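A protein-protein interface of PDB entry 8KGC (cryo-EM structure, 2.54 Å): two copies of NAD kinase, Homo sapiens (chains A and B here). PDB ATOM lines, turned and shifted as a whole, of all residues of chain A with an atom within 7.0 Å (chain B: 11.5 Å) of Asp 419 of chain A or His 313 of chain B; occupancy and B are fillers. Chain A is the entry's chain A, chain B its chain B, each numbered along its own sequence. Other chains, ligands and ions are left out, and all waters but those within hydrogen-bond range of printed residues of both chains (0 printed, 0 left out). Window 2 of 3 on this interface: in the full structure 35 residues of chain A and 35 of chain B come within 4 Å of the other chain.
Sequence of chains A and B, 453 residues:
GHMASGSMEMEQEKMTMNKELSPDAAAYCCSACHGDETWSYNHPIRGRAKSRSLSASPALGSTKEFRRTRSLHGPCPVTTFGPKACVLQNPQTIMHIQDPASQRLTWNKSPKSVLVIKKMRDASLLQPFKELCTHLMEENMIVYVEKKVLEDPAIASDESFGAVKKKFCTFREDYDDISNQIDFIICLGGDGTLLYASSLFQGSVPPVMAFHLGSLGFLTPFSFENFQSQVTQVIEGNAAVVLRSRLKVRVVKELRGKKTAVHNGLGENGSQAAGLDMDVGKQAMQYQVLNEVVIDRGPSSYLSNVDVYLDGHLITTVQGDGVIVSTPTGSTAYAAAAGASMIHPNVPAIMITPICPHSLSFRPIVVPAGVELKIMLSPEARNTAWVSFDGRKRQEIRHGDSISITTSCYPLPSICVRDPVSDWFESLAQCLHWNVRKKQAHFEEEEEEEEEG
OD2 of Asp 419 of chain A is in hydrogen-bond range of OG of Ser 422 of chain A, at 2.6 Å.
O of Ile 352 of chain B is in hydrogen-bond range of N of Ile 365 of chain B (2.9 Å).
The backbone carbonyl oxygen of Val 308 of chain B is in hydrogen-bond range of the backbone NH of Ile 315 of chain B (2.9 Å).
No position is printed for both chains.
Of the 7 pairs that touch across the chains among the printed residues, none has its exchanged pair printed and touching as well.
Among the printed residues, merely in contact across the chains: His 344 of chain A with Pro 368 of chain B (3.7 Å), Asp 419 of chain A with His 313 of chain B (3.4 Å), Val 421 of chain A with Leu 310 of chain B (3.6 Å), Trp 424 of chain A with Ile 365 of chain B (3.5 Å), Phe 425 of chain A with Leu 310 of chain B (3.6 Å) and Phe 425 of chain A with Ile 315 of chain B (3.5 Å).
Of the 13 printed residues of chain A, 6 touch a printed residue of chain B.
Among the printed residues, no Asp or Glu carboxylate lies within 4 Å of a Lys or Arg side-chain nitrogen of the other chain.
The side-chain hydroxyl (OG) of Ser 422 of chain A lies within hydrogen-bond range of a ring nitrogen (ND1) of His 313 of chain B, at 2.7 Å.
Printed residues of chain B within 4 Å of Asp 419 of chain A: His 313 (3.4 Å).
No residue of chain B comes within 4 Å of Cys 416 of chain A.
No residue of chain B comes within 4 Å of Val 417 of chain A.
No residue of chain B comes within 4 Å of Arg 418 of chain A.
No residue of chain B comes within 4 Å of Pro 420 of chain A.
Val 421 of chain A touches one residue of chain B.
Of the printed residues of chain A, Ile 365 of chain B touches Trp 424.
Of the printed residues of chain B, Trp 424 of chain A touches Ile 365 (3.5 Å).
Printed residues of chain B within 4 Å of His 344 of chain A: Pro 368.
Of the printed residues of chain A, Pro 368 of chain B touches His 344.
Ile 375 of chain B touches none of the printed residues of chain A.
The nearest residue of chain B that does not touch Asp 419 of chain A is Asp 311 of chain B (6.6 Å).
The nearest residue of chain A that does not touch His 313 of chain B is Val 421 of chain A (5.4 Å).
The nearest printed residue of chain B that does not touch Phe 425 of chain A is Ile 365 of chain B (4.4 Å).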
ATOM      1  N   ALA A 240      20.835 -29.280  -0.267  1.00  0.00           N
ATOM      2  CA  ALA A 240      21.854 -29.231  -1.303  1.00  0.00           C
ATOM      3  C   ALA A 240      22.766 -28.028  -1.104  1.00  0.00           C
ATOM      4  O   ALA A 240      22.365 -27.000  -0.552  1.00  0.00           O
ATOM      5  CB  ALA A 240      21.211 -29.177  -2.689  1.00  0.00           C
ATOM      6  N   VAL A 242      25.882 -25.582  -3.039  1.00  0.00           N
ATOM      7  CA  VAL A 242      26.638 -25.138  -4.205  1.00  0.00           C
ATOM      8  C   VAL A 242      27.938 -24.524  -3.708  1.00  0.00           C
ATOM      9  O   VAL A 242      27.919 -23.586  -2.902  1.00  0.00           O
ATOM     10  CB  VAL A 242      25.848 -24.129  -5.050  1.00  0.00           C
ATOM     11  CG1 VAL A 242      26.770 -23.430  -6.030  1.00  0.00           C
ATOM     12  CG2 VAL A 242      24.736 -24.823  -5.792  1.00  0.00           C
ATOM     13  N   HIS A 344      26.530 -21.206 -15.080  1.00  0.00           N
ATOM     14  CA  HIS A 344      26.094 -21.903 -13.883  1.00  0.00           C
ATOM     15  C   HIS A 344      27.229 -21.940 -12.862  1.00  0.00           C
ATOM     16  O   HIS A 344      28.382 -22.186 -13.226  1.00  0.00           O
ATOM     17  CB  HIS A 344      25.650 -23.322 -14.230  1.00  0.00           C
ATOM     18  CG  HIS A 344      24.950 -24.029 -13.112  1.00  0.00           C
ATOM     19  ND1 HIS A 344      25.625 -24.610 -12.061  1.00  0.00           N
ATOM     20  CD2 HIS A 344      23.635 -24.256 -12.886  1.00  0.00           C
ATOM     21  CE1 HIS A 344      24.756 -25.160 -11.234  1.00  0.00           C
ATOM     22  NE2 HIS A 344      23.541 -24.959 -11.711  1.00  0.00           N
ATOM     23  N   CYS A 416      21.079 -24.629  -0.889  1.00  0.00           N
ATOM     24  CA  CYS A 416      20.077 -24.570  -1.942  1.00  0.00           C
ATOM     25  C   CYS A 416      18.702 -24.926  -1.395  1.00  0.00           C
ATOM     26  O   CYS A 416      18.576 -25.647  -0.402  1.00  0.00           O
ATOM     27  CB  CYS A 416      20.434 -25.522  -3.083  1.00  0.00           C
ATOM     28  SG  CYS A 416      22.172 -25.504  -3.538  1.00  0.00           S
ATOM     29  N   VAL A 417      17.666 -24.414  -2.059  1.00  0.00           N
ATOM     30  CA  VAL A 417      16.298 -24.746  -1.670  1.00  0.00           C
ATOM     31  C   VAL A 417      15.967 -26.178  -2.072  1.00  0.00           C
ATOM     32  O   VAL A 417      15.669 -27.027  -1.225  1.00  0.00           O
ATOM     33  CB  VAL A 417      15.302 -23.748  -2.285  1.00  0.00           C
ATOM     34  CG1 VAL A 417      13.877 -24.179  -1.988  1.00  0.00           C
ATOM     35  CG2 VAL A 417      15.556 -22.354  -1.750  1.00  0.00           C
ATOM     36  N   ARG A 418      16.015 -26.466  -3.372  1.00  0.00           N
ATOM     37  CA  ARG A 418      15.721 -27.804  -3.874  1.00  0.00           C
ATOM     38  C   ARG A 418      16.929 -28.448  -4.541  1.00  0.00           C
ATOM     39  O   ARG A 418      17.334 -29.544  -4.140  1.00  0.00           O
ATOM     40  CB  ARG A 418      14.529 -27.750  -4.837  1.00  0.00           C
ATOM     41  CG  ARG A 418      14.331 -26.402  -5.505  1.00  0.00           C
ATOM     42  CD  ARG A 418      13.052 -26.385  -6.324  1.00  0.00           C
ATOM     43  NE  ARG A 418      12.707 -25.041  -6.770  1.00  0.00           N
ATOM     44  CZ  ARG A 418      11.934 -24.204  -6.091  1.00  0.00           C
ATOM     45  N   ASP A 419      17.518 -27.807  -5.546  1.00  0.00           N
ATOM     46  CA  ASP A 419      18.689 -28.343  -6.226  1.00  0.00           C
ATOM     47  C   ASP A 419      19.393 -27.198  -6.941  1.00  0.00           C
ATOM     48  O   ASP A 419      18.772 -26.167  -7.223  1.00  0.00           O
ATOM     49  CB  ASP A 419      18.302 -29.453  -7.217  1.00  0.00           C
ATOM     50  CG  ASP A 419      17.119 -29.078  -8.079  1.00  0.00           C
ATOM     51  OD1 ASP A 419      16.150 -28.513  -7.535  1.00  0.00           O
ATOM     52  OD2 ASP A 419      17.158 -29.346  -9.297  1.00  0.00           O
ATOM     53  N   PRO A 420      20.688 -27.346  -7.236  1.00  0.00           N
ATOM     54  CA  PRO A 420      21.418 -26.233  -7.875  1.00  0.00           C
ATOM     55  C   PRO A 420      20.824 -25.782  -9.198  1.00  0.00           C
ATOM     56  O   PRO A 420      20.636 -24.577  -9.412  1.00  0.00           O
ATOM     57  CB  PRO A 420      22.828 -26.811  -8.053  1.00  0.00           C
ATOM     58  CG  PRO A 420      22.946 -27.846  -6.995  1.00  0.00           C
ATOM     59  CD  PRO A 420      21.585 -28.456  -6.874  1.00  0.00           C
ATOM     60  N   VAL A 421      20.518 -26.720 -10.095  1.00  0.00           N
ATOM     61  CA  VAL A 421      20.064 -26.358 -11.434  1.00  0.00           C
ATOM     62  C   VAL A 421      18.721 -25.638 -11.375  1.00  0.00           C
ATOM     63  O   VAL A 421      18.544 -24.566 -11.967  1.00  0.00           O
ATOM     64  CB  VAL A 421      19.992 -27.612 -12.324  1.00  0.00           C
ATOM     65  CG1 VAL A 421      19.295 -27.294 -13.629  1.00  0.00           C
ATOM     66  CG2 VAL A 421      21.386 -28.161 -12.576  1.00  0.00           C
ATOM     67  N   SER A 422      17.754 -26.220 -10.662  1.00  0.00           N
ATOM     68  CA  SER A 422      16.423 -25.628 -10.609  1.00  0.00           C
ATOM     69  C   SER A 422      16.448 -24.270  -9.926  1.00  0.00           C
ATOM     70  O   SER A 422      15.810 -23.322 -10.395  1.00  0.00           O
ATOM     71  CB  SER A 422      15.455 -26.568  -9.895  1.00  0.00           C
ATOM     72  OG  SER A 422      15.401 -27.829 -10.540  1.00  0.00           O
ATOM     73  N   ASP A 423      17.181 -24.154  -8.816  1.00  0.00           N
ATOM     74  CA  ASP A 423      17.277 -22.870  -8.130  1.00  0.00           C
ATOM     75  C   ASP A 423      17.930 -21.822  -9.016  1.00  0.00           C
ATOM     76  O   ASP A 423      17.466 -20.676  -9.081  1.00  0.00           O
ATOM     77  CB  ASP A 423      18.058 -23.022  -6.827  1.00  0.00           C
ATOM     78  CG  ASP A 423      17.184 -23.445  -5.670  1.00  0.00           C
ATOM     79  OD1 ASP A 423      15.961 -23.595  -5.870  1.00  0.00           O
ATOM     80  OD2 ASP A 423      17.720 -23.621  -4.556  1.00  0.00           O
ATOM     81  N   TRP A 424      19.009 -22.193  -9.706  1.00  0.00           N
ATOM     82  CA  TRP A 424      19.695 -21.231 -10.558  1.00  0.00           C
ATOM     83  C   TRP A 424      18.794 -20.759 -11.688  1.00  0.00           C
ATOM     84  O   TRP A 424      18.739 -19.562 -11.984  1.00  0.00           O
ATOM     85  CB  TRP A 424      20.982 -21.834 -11.114  1.00  0.00           C
ATOM     86  CG  TRP A 424      21.779 -20.853 -11.904  1.00  0.00           C
ATOM     87  CD1 TRP A 424      22.368 -19.715 -11.438  1.00  0.00           C
ATOM     88  CD2 TRP A 424      22.078 -20.915 -13.301  1.00  0.00           C
ATOM     89  NE1 TRP A 424      23.014 -19.065 -12.458  1.00  0.00           N
ATOM     90  CE2 TRP A 424      22.852 -19.782 -13.613  1.00  0.00           C
ATOM     91  CE3 TRP A 424      21.768 -21.821 -14.318  1.00  0.00           C
ATOM     92  CZ2 TRP A 424      23.318 -19.531 -14.896  1.00  0.00           C
ATOM     93  CZ3 TRP A 424      22.232 -21.568 -15.591  1.00  0.00           C
ATOM     94  CH2 TRP A 424      22.998 -20.433 -15.869  1.00  0.00           C
ATOM     95  N   PHE A 425      18.060 -21.678 -12.319  1.00  0.00           N
ATOM     96  CA  PHE A 425      17.200 -21.268 -13.425  1.00  0.00           C
ATOM     97  C   PHE A 425      16.001 -20.467 -12.936  1.00  0.00           C
ATOM     98  O   PHE A 425      15.562 -19.529 -13.611  1.00  0.00           O
ATOM     99  CB  PHE A 425      16.756 -22.484 -14.232  1.00  0.00           C
ATOM    100  CG  PHE A 425      17.793 -22.961 -15.200  1.00  0.00           C
ATOM    101  CD1 PHE A 425      18.189 -22.158 -16.252  1.00  0.00           C
ATOM    102  CD2 PHE A 425      18.379 -24.203 -15.056  1.00  0.00           C
ATOM    103  CE1 PHE A 425      19.150 -22.585 -17.142  1.00  0.00           C
ATOM    104  CE2 PHE A 425      19.339 -24.637 -15.946  1.00  0.00           C
ATOM    105  CZ  PHE A 425      19.725 -23.827 -16.989  1.00  0.00           C
ATOM    106  N   VAL B 306      10.936 -25.176 -29.836  1.00  0.00           N
ATOM    107  CA  VAL B 306      11.343 -26.417 -29.188  1.00  0.00           C
ATOM    108  C   VAL B 306      11.415 -26.194 -27.682  1.00  0.00           C
ATOM    109  O   VAL B 306      11.407 -25.065 -27.198  1.00  0.00           O
ATOM    110  CB  VAL B 306      12.688 -26.943 -29.724  1.00  0.00           C
ATOM    111  CG1 VAL B 306      12.584 -27.241 -31.207  1.00  0.00           C
ATOM    112  CG2 VAL B 306      13.790 -25.939 -29.457  1.00  0.00           C
ATOM    113  N   ASP B 307      11.489 -27.297 -26.942  1.00  0.00           N
ATOM    114  CA  ASP B 307      11.589 -27.273 -25.490  1.00  0.00           C
ATOM    115  C   ASP B 307      12.895 -27.925 -25.066  1.00  0.00           C
ATOM    116  O   ASP B 307      13.234 -29.018 -25.540  1.00  0.00           O
ATOM    117  CB  ASP B 307      10.406 -27.993 -24.838  1.00  0.00           C
ATOM    118  CG  ASP B 307       9.103 -27.241 -25.005  1.00  0.00           C
ATOM    119  OD1 ASP B 307       9.148 -26.007 -25.194  1.00  0.00           O
ATOM    120  OD2 ASP B 307       8.033 -27.881 -24.941  1.00  0.00           O
ATOM    121  N   VAL B 308      13.621 -27.255 -24.175  1.00  0.00           N
ATOM    122  CA  VAL B 308      14.888 -27.738 -23.644  1.00  0.00           C
ATOM    123  C   VAL B 308      14.674 -28.094 -22.182  1.00  0.00           C
ATOM    124  O   VAL B 308      14.200 -27.260 -21.394  1.00  0.00           O
ATOM    125  CB  VAL B 308      16.003 -26.693 -23.797  1.00  0.00           C
ATOM    126  CG1 VAL B 308      17.311 -27.235 -23.251  1.00  0.00           C
ATOM    127  CG2 VAL B 308      16.152 -26.287 -25.249  1.00  0.00           C
ATOM    128  N   TYR B 309      15.019 -29.333 -21.832  1.00  0.00           N
ATOM    129  CA  TYR B 309      14.988 -29.855 -20.475  1.00  0.00           C
ATOM    130  C   TYR B 309      16.414 -30.111 -20.012  1.00  0.00           C
ATOM    131  O   TYR B 309      17.261 -30.547 -20.799  1.00  0.00           O
ATOM    132  CB  TYR B 309      14.200 -31.166 -20.396  1.00  0.00           C
ATOM    133  CG  TYR B 309      12.751 -31.084 -20.814  1.00  0.00           C
ATOM    134  CD1 TYR B 309      12.396 -30.979 -22.150  1.00  0.00           C
ATOM    135  CD2 TYR B 309      11.736 -31.148 -19.871  1.00  0.00           C
ATOM    136  CE1 TYR B 309      11.075 -30.914 -22.534  1.00  0.00           C
ATOM    137  CE2 TYR B 309      10.411 -31.084 -20.244  1.00  0.00           C
ATOM    138  CZ  TYR B 309      10.086 -30.968 -21.577  1.00  0.00           C
ATOM    139  OH  TYR B 309       8.765 -30.906 -21.954  1.00  0.00           O
ATOM    140  N   LEU B 310      16.674 -29.861 -18.732  1.00  0.00           N
ATOM    141  CA  LEU B 310      17.981 -30.115 -18.139  1.00  0.00           C
ATOM    142  C   LEU B 310      17.782 -31.002 -16.921  1.00  0.00           C
ATOM    143  O   LEU B 310      17.132 -30.594 -15.954  1.00  0.00           O
ATOM    144  CB  LEU B 310      18.677 -28.806 -17.757  1.00  0.00           C
ATOM    145  CG  LEU B 310      20.200 -28.807 -17.645  1.00  0.00           C
ATOM    146  CD1 LEU B 310      20.734 -27.401 -17.835  1.00  0.00           C
ATOM    147  CD2 LEU B 310      20.646 -29.362 -16.307  1.00  0.00           C
ATOM    148  N   ASP B 311      18.339 -32.214 -16.974  1.00  0.00           N
ATOM    149  CA  ASP B 311      18.200 -33.199 -15.900  1.00  0.00           C
ATOM    150  C   ASP B 311      16.732 -33.475 -15.583  1.00  0.00           C
ATOM    151  O   ASP B 311      16.346 -33.631 -14.423  1.00  0.00           O
ATOM    152  CB  ASP B 311      18.955 -32.762 -14.643  1.00  0.00           C
ATOM    153  CG  ASP B 311      20.457 -32.885 -14.794  1.00  0.00           C
ATOM    154  OD1 ASP B 311      20.909 -33.775 -15.545  1.00  0.00           O
ATOM    155  OD2 ASP B 311      21.187 -32.097 -14.157  1.00  0.00           O
ATOM    156  N   GLY B 312      15.904 -33.534 -16.623  1.00  0.00           N
ATOM    157  CA  GLY B 312      14.498 -33.828 -16.467  1.00  0.00           C
ATOM    158  C   GLY B 312      13.622 -32.644 -16.127  1.00  0.00           C
ATOM    159  O   GLY B 312      12.398 -32.807 -16.037  1.00  0.00           O
ATOM    160  N   HIS B 313      14.199 -31.462 -15.936  1.00  0.00           N
ATOM    161  CA  HIS B 313      13.449 -30.254 -15.626  1.00  0.00           C
ATOM    162  C   HIS B 313      13.435 -29.352 -16.849  1.00  0.00           C
ATOM    163  O   HIS B 313      14.480 -29.122 -17.465  1.00  0.00           O
ATOM    164  CB  HIS B 313      14.062 -29.518 -14.433  1.00  0.00           C
ATOM    165  CG  HIS B 313      14.108 -30.334 -13.180  1.00  0.00           C
ATOM    166  ND1 HIS B 313      14.916 -30.013 -12.111  1.00  0.00           N
ATOM    167  CD2 HIS B 313      13.442 -31.458 -12.823  1.00  0.00           C
ATOM    168  CE1 HIS B 313      14.749 -30.905 -11.151  1.00  0.00           C
ATOM    169  NE2 HIS B 313      13.860 -31.792 -11.559  1.00  0.00           N
ATOM    170  N   LEU B 314      12.260 -28.831 -17.187  1.00  0.00           N
ATOM    171  CA  LEU B 314      12.105 -28.008 -18.384  1.00  0.00           C
ATOM    172  C   LEU B 314      12.790 -26.673 -18.143  1.00  0.00           C
ATOM    173  O   LEU B 314      12.205 -25.754 -17.567  1.00  0.00           O
ATOM    174  CB  LEU B 314      10.628 -27.820 -18.710  1.00  0.00           C
ATOM    175  CG  LEU B 314      10.292 -26.921 -19.901  1.00  0.00           C
ATOM    176  CD1 LEU B 314      10.830 -27.515 -21.189  1.00  0.00           C
ATOM    177  CD2 LEU B 314       8.793 -26.694 -19.996  1.00  0.00           C
ATOM    178  N   ILE B 315      14.048 -26.563 -18.573  1.00  0.00           N
ATOM    179  CA  ILE B 315      14.784 -25.324 -18.352  1.00  0.00           C
ATOM    180  C   ILE B 315      14.175 -24.185 -19.157  1.00  0.00           C
ATOM    181  O   ILE B 315      13.953 -23.092 -18.623  1.00  0.00           O
ATOM    182  CB  ILE B 315      16.284 -25.503 -18.664  1.00  0.00           C
ATOM    183  CG1 ILE B 315      16.868 -24.221 -19.264  1.00  0.00           C
ATOM    184  CG2 ILE B 315      16.520 -26.674 -19.580  1.00  0.00           C
ATOM    185  CD1 ILE B 315      18.156 -24.430 -20.034  1.00  0.00           C
ATOM    186  N   THR B 316      13.871 -24.409 -20.435  1.00  0.00           N
ATOM    187  CA  THR B 316      13.420 -23.276 -21.237  1.00  0.00           C
ATOM    188  C   THR B 316      12.680 -23.758 -22.477  1.00  0.00           C
ATOM    189  O   THR B 316      12.588 -24.955 -22.758  1.00  0.00           O
ATOM    190  CB  THR B 316      14.593 -22.378 -21.635  1.00  0.00           C
ATOM    191  OG1 THR B 316      14.097 -21.228 -22.331  1.00  0.00           O
ATOM    192  CG2 THR B 316      15.551 -23.128 -22.542  1.00  0.00           C
ATOM    193  N   THR B 317      12.148 -22.790 -23.220  1.00  0.00           N
ATOM    194  CA  THR B 317      11.544 -23.007 -24.525  1.00  0.00           C
ATOM    195  C   THR B 317      12.203 -22.059 -25.514  1.00  0.00           C
ATOM    196  O   THR B 317      12.212 -20.843 -25.300  1.00  0.00           O
ATOM    197  CB  THR B 317      10.031 -22.774 -24.489  1.00  0.00           C
ATOM    198  OG1 THR B 317       9.409 -23.784 -23.687  1.00  0.00           O
ATOM    199  CG2 THR B 317       9.450 -22.814 -25.891  1.00  0.00           C
ATOM    200  N   VAL B 318      12.750 -22.613 -26.588  1.00  0.00           N
ATOM    201  CA  VAL B 318      13.467 -21.846 -27.598  1.00  0.00           C
ATOM    202  C   VAL B 318      12.514 -21.556 -28.746  1.00  0.00           C
ATOM    203  O   VAL B 318      11.987 -22.481 -29.377  1.00  0.00           O
ATOM    204  CB  VAL B 318      14.711 -22.596 -28.095  1.00  0.00           C
ATOM    205  CG1 VAL B 318      15.383 -21.817 -29.210  1.00  0.00           C
ATOM    206  CG2 VAL B 318      15.677 -22.835 -26.947  1.00  0.00           C
ATOM    207  N   ILE B 352      24.905 -23.350 -24.447  1.00  0.00           N
ATOM    208  CA  ILE B 352      23.615 -23.298 -25.124  1.00  0.00           C
ATOM    209  C   ILE B 352      23.455 -21.896 -25.686  1.00  0.00           C
ATOM    210  O   ILE B 352      23.414 -20.921 -24.928  1.00  0.00           O
ATOM    211  CB  ILE B 352      22.457 -23.642 -24.178  1.00  0.00           C
ATOM    212  CG1 ILE B 352      22.683 -25.002 -23.525  1.00  0.00           C
ATOM    213  CG2 ILE B 352      21.141 -23.629 -24.928  1.00  0.00           C
ATOM    214  CD1 ILE B 352      21.674 -25.325 -22.458  1.00  0.00           C
ATOM    215  N   ILE B 365      23.816 -19.536 -22.426  1.00  0.00           N
ATOM    216  CA  ILE B 365      24.015 -20.198 -21.146  1.00  0.00           C
ATOM    217  C   ILE B 365      25.273 -21.047 -21.217  1.00  0.00           C
ATOM    218  O   ILE B 365      25.647 -21.559 -22.278  1.00  0.00           O
ATOM    219  CB  ILE B 365      22.814 -21.082 -20.756  1.00  0.00           C
ATOM    220  CG1 ILE B 365      21.517 -20.536 -21.339  1.00  0.00           C
ATOM    221  CG2 ILE B 365      22.703 -21.199 -19.253  1.00  0.00           C
ATOM    222  CD1 ILE B 365      20.401 -21.547 -21.303  1.00  0.00           C
ATOM    223  N   VAL B 367      26.589 -24.338 -18.931  1.00  0.00           N
ATOM    224  CA  VAL B 367      26.096 -25.274 -17.925  1.00  0.00           C
ATOM    225  C   VAL B 367      27.194 -26.291 -17.660  1.00  0.00           C
ATOM    226  O   VAL B 367      28.103 -26.476 -18.488  1.00  0.00           O
ATOM    227  CB  VAL B 367      24.778 -25.950 -18.370  1.00  0.00           C
ATOM    228  CG1 VAL B 367      23.708 -24.905 -18.617  1.00  0.00           C
ATOM    229  CG2 VAL B 367      25.004 -26.782 -19.613  1.00  0.00           C
ATOM    230  N   PRO B 368      27.159 -26.958 -16.506  1.00  0.00           N
ATOM    231  CA  PRO B 368      28.207 -27.935 -16.192  1.00  0.00           C
ATOM    232  C   PRO B 368      28.217 -29.087 -17.183  1.00  0.00           C
ATOM    233  O   PRO B 368      27.193 -29.445 -17.767  1.00  0.00           O
ATOM    234  CB  PRO B 368      27.836 -28.416 -14.785  1.00  0.00           C
ATOM    235  CG  PRO B 368      27.002 -27.330 -14.223  1.00  0.00           C
ATOM    236  CD  PRO B 368      26.241 -26.761 -15.372  1.00  0.00           C
ATOM    237  N   VAL B 371      25.764 -32.398 -16.821  1.00  0.00           N
ATOM    238  CA  VAL B 371      24.316 -32.366 -16.988  1.00  0.00           C
ATOM    239  C   VAL B 371      23.925 -33.171 -18.219  1.00  0.00           C
ATOM    240  O   VAL B 371      24.779 -33.542 -19.030  1.00  0.00           O
ATOM    241  CB  VAL B 371      23.798 -30.923 -17.094  1.00  0.00           C
ATOM    242  CG1 VAL B 371      24.309 -30.091 -15.933  1.00  0.00           C
ATOM    243  CG2 VAL B 371      24.203 -30.313 -18.419  1.00  0.00           C
ATOM    244  N   GLU B 372      22.631 -33.451 -18.362  1.00  0.00           N
ATOM    245  CA  GLU B 372      22.098 -34.197 -19.500  1.00  0.00           C
ATOM    246  C   GLU B 372      20.967 -33.383 -20.118  1.00  0.00           C
ATOM    247  O   GLU B 372      19.851 -33.359 -19.592  1.00  0.00           O
ATOM    248  CB  GLU B 372      21.616 -35.579 -19.074  1.00  0.00           C
ATOM    249  CG  GLU B 372      20.878 -36.337 -20.164  1.00  0.00           C
ATOM    250  CD  GLU B 372      20.430 -37.711 -19.715  1.00  0.00           C
ATOM    251  OE1 GLU B 372      20.804 -38.123 -18.597  1.00  0.00           O
ATOM    252  OE2 GLU B 372      19.702 -38.381 -20.479  1.00  0.00           O
ATOM    253  N   LEU B 373      21.253 -32.717 -21.233  1.00  0.00           N
ATOM    254  CA  LEU B 373      20.232 -31.964 -21.940  1.00  0.00           C
ATOM    255  C   LEU B 373      19.302 -32.898 -22.698  1.00  0.00           C
ATOM    256  O   LEU B 373      19.708 -33.958 -23.178  1.00  0.00           O
ATOM    257  CB  LEU B 373      20.860 -30.979 -22.924  1.00  0.00           C
ATOM    258  CG  LEU B 373      21.267 -29.603 -22.412  1.00  0.00           C
ATOM    259  CD1 LEU B 373      22.480 -29.699 -21.516  1.00  0.00           C
ATOM    260  CD2 LEU B 373      21.539 -28.692 -23.588  1.00  0.00           C
ATOM    261  N   LYS B 374      18.044 -32.484 -22.818  1.00  0.00           N
ATOM    262  CA  LYS B 374      17.067 -33.199 -23.630  1.00  0.00           C
ATOM    263  C   LYS B 374      16.249 -32.173 -24.395  1.00  0.00           C
ATOM    264  O   LYS B 374      15.538 -31.366 -23.791  1.00  0.00           O
ATOM    265  CB  LYS B 374      16.161 -34.082 -22.768  1.00  0.00           C
ATOM    266  CG  LYS B 374      15.165 -34.902 -23.566  1.00  0.00           C
ATOM    267  CD  LYS B 374      14.341 -35.801 -22.662  1.00  0.00           C
ATOM    268  N   ILE B 375      16.349 -32.200 -25.717  1.00  0.00           N
ATOM    269  CA  ILE B 375      15.651 -31.260 -26.581  1.00  0.00           C
ATOM    270  C   ILE B 375      14.532 -32.006 -27.291  1.00  0.00           C
ATOM    271  O   ILE B 375      14.762 -33.070 -27.881  1.00  0.00           O
ATOM    272  CB  ILE B 375      16.608 -30.604 -27.590  1.00  0.00           C
ATOM    273  CG1 ILE B 375      17.715 -29.856 -26.849  1.00  0.00           C
ATOM    274  CG2 ILE B 375      15.851 -29.659 -28.501  1.00  0.00           C
ATOM    275  CD1 ILE B 375      18.675 -29.138 -27.761  1.00  0.00           C
ATOM    276  N   MET B 376      13.321 -31.458 -27.218  1.00  0.00           N
ATOM    277  CA  MET B 376      12.165 -32.061 -27.862  1.00  0.00           C
ATOM    278  C   MET B 376      11.358 -30.980 -28.559  1.00  0.00           C
ATOM    279  O   MET B 376      11.593 -29.784 -28.382  1.00  0.00           O
ATOM    280  CB  MET B 376      11.281 -32.813 -26.860  1.00  0.00           C
ATOM    281  CG  MET B 376      11.964 -33.970 -26.161  1.00  0.00           C
ATOM    282  SD  MET B 376      10.797 -35.026 -25.283  1.00  0.00           S
ATOM    283  CE  MET B 376       9.926 -33.815 -24.295  1.00  0.00           C
ATOM    284  N   ILE B 403      16.244 -35.548 -28.404  1.00  0.00           N
ATOM    285  CA  ILE B 403      17.688 -35.464 -28.578  1.00  0.00           C
ATOM    286  C   ILE B 403      18.304 -35.347 -27.192  1.00  0.00           C
ATOM    287  O   ILE B 403      18.095 -34.344 -26.501  1.00  0.00           O
ATOM    288  CB  ILE B 403      18.089 -34.274 -29.459  1.00  0.00           C
ATOM    289  CG1 ILE B 403      17.420 -34.378 -30.830  1.00  0.00           C
ATOM    290  CG2 ILE B 403      19.592 -34.203 -29.604  1.00  0.00           C
ATOM    291  CD1 ILE B 403      17.687 -33.193 -31.722  1.00  0.00           C
ATOM    292  N   ILE B 405      21.681 -35.046 -24.990  1.00  0.00           N
ATOM    293  CA  ILE B 405      23.046 -34.563 -25.155  1.00  0.00           C
ATOM    294  C   ILE B 405      23.755 -34.635 -23.813  1.00  0.00           C
ATOM    295  O   ILE B 405      23.268 -34.084 -22.819  1.00  0.00           O
ATOM    296  CB  ILE B 405      23.074 -33.126 -25.705  1.00  0.00           C
ATOM    297  CG1 ILE B 405      22.300 -33.048 -27.021  1.00  0.00           C
ATOM    298  CG2 ILE B 405      24.502 -32.661 -25.896  1.00  0.00           C
ATOM    299  CD1 ILE B 405      22.208 -31.656 -27.587  1.00  0.00           C
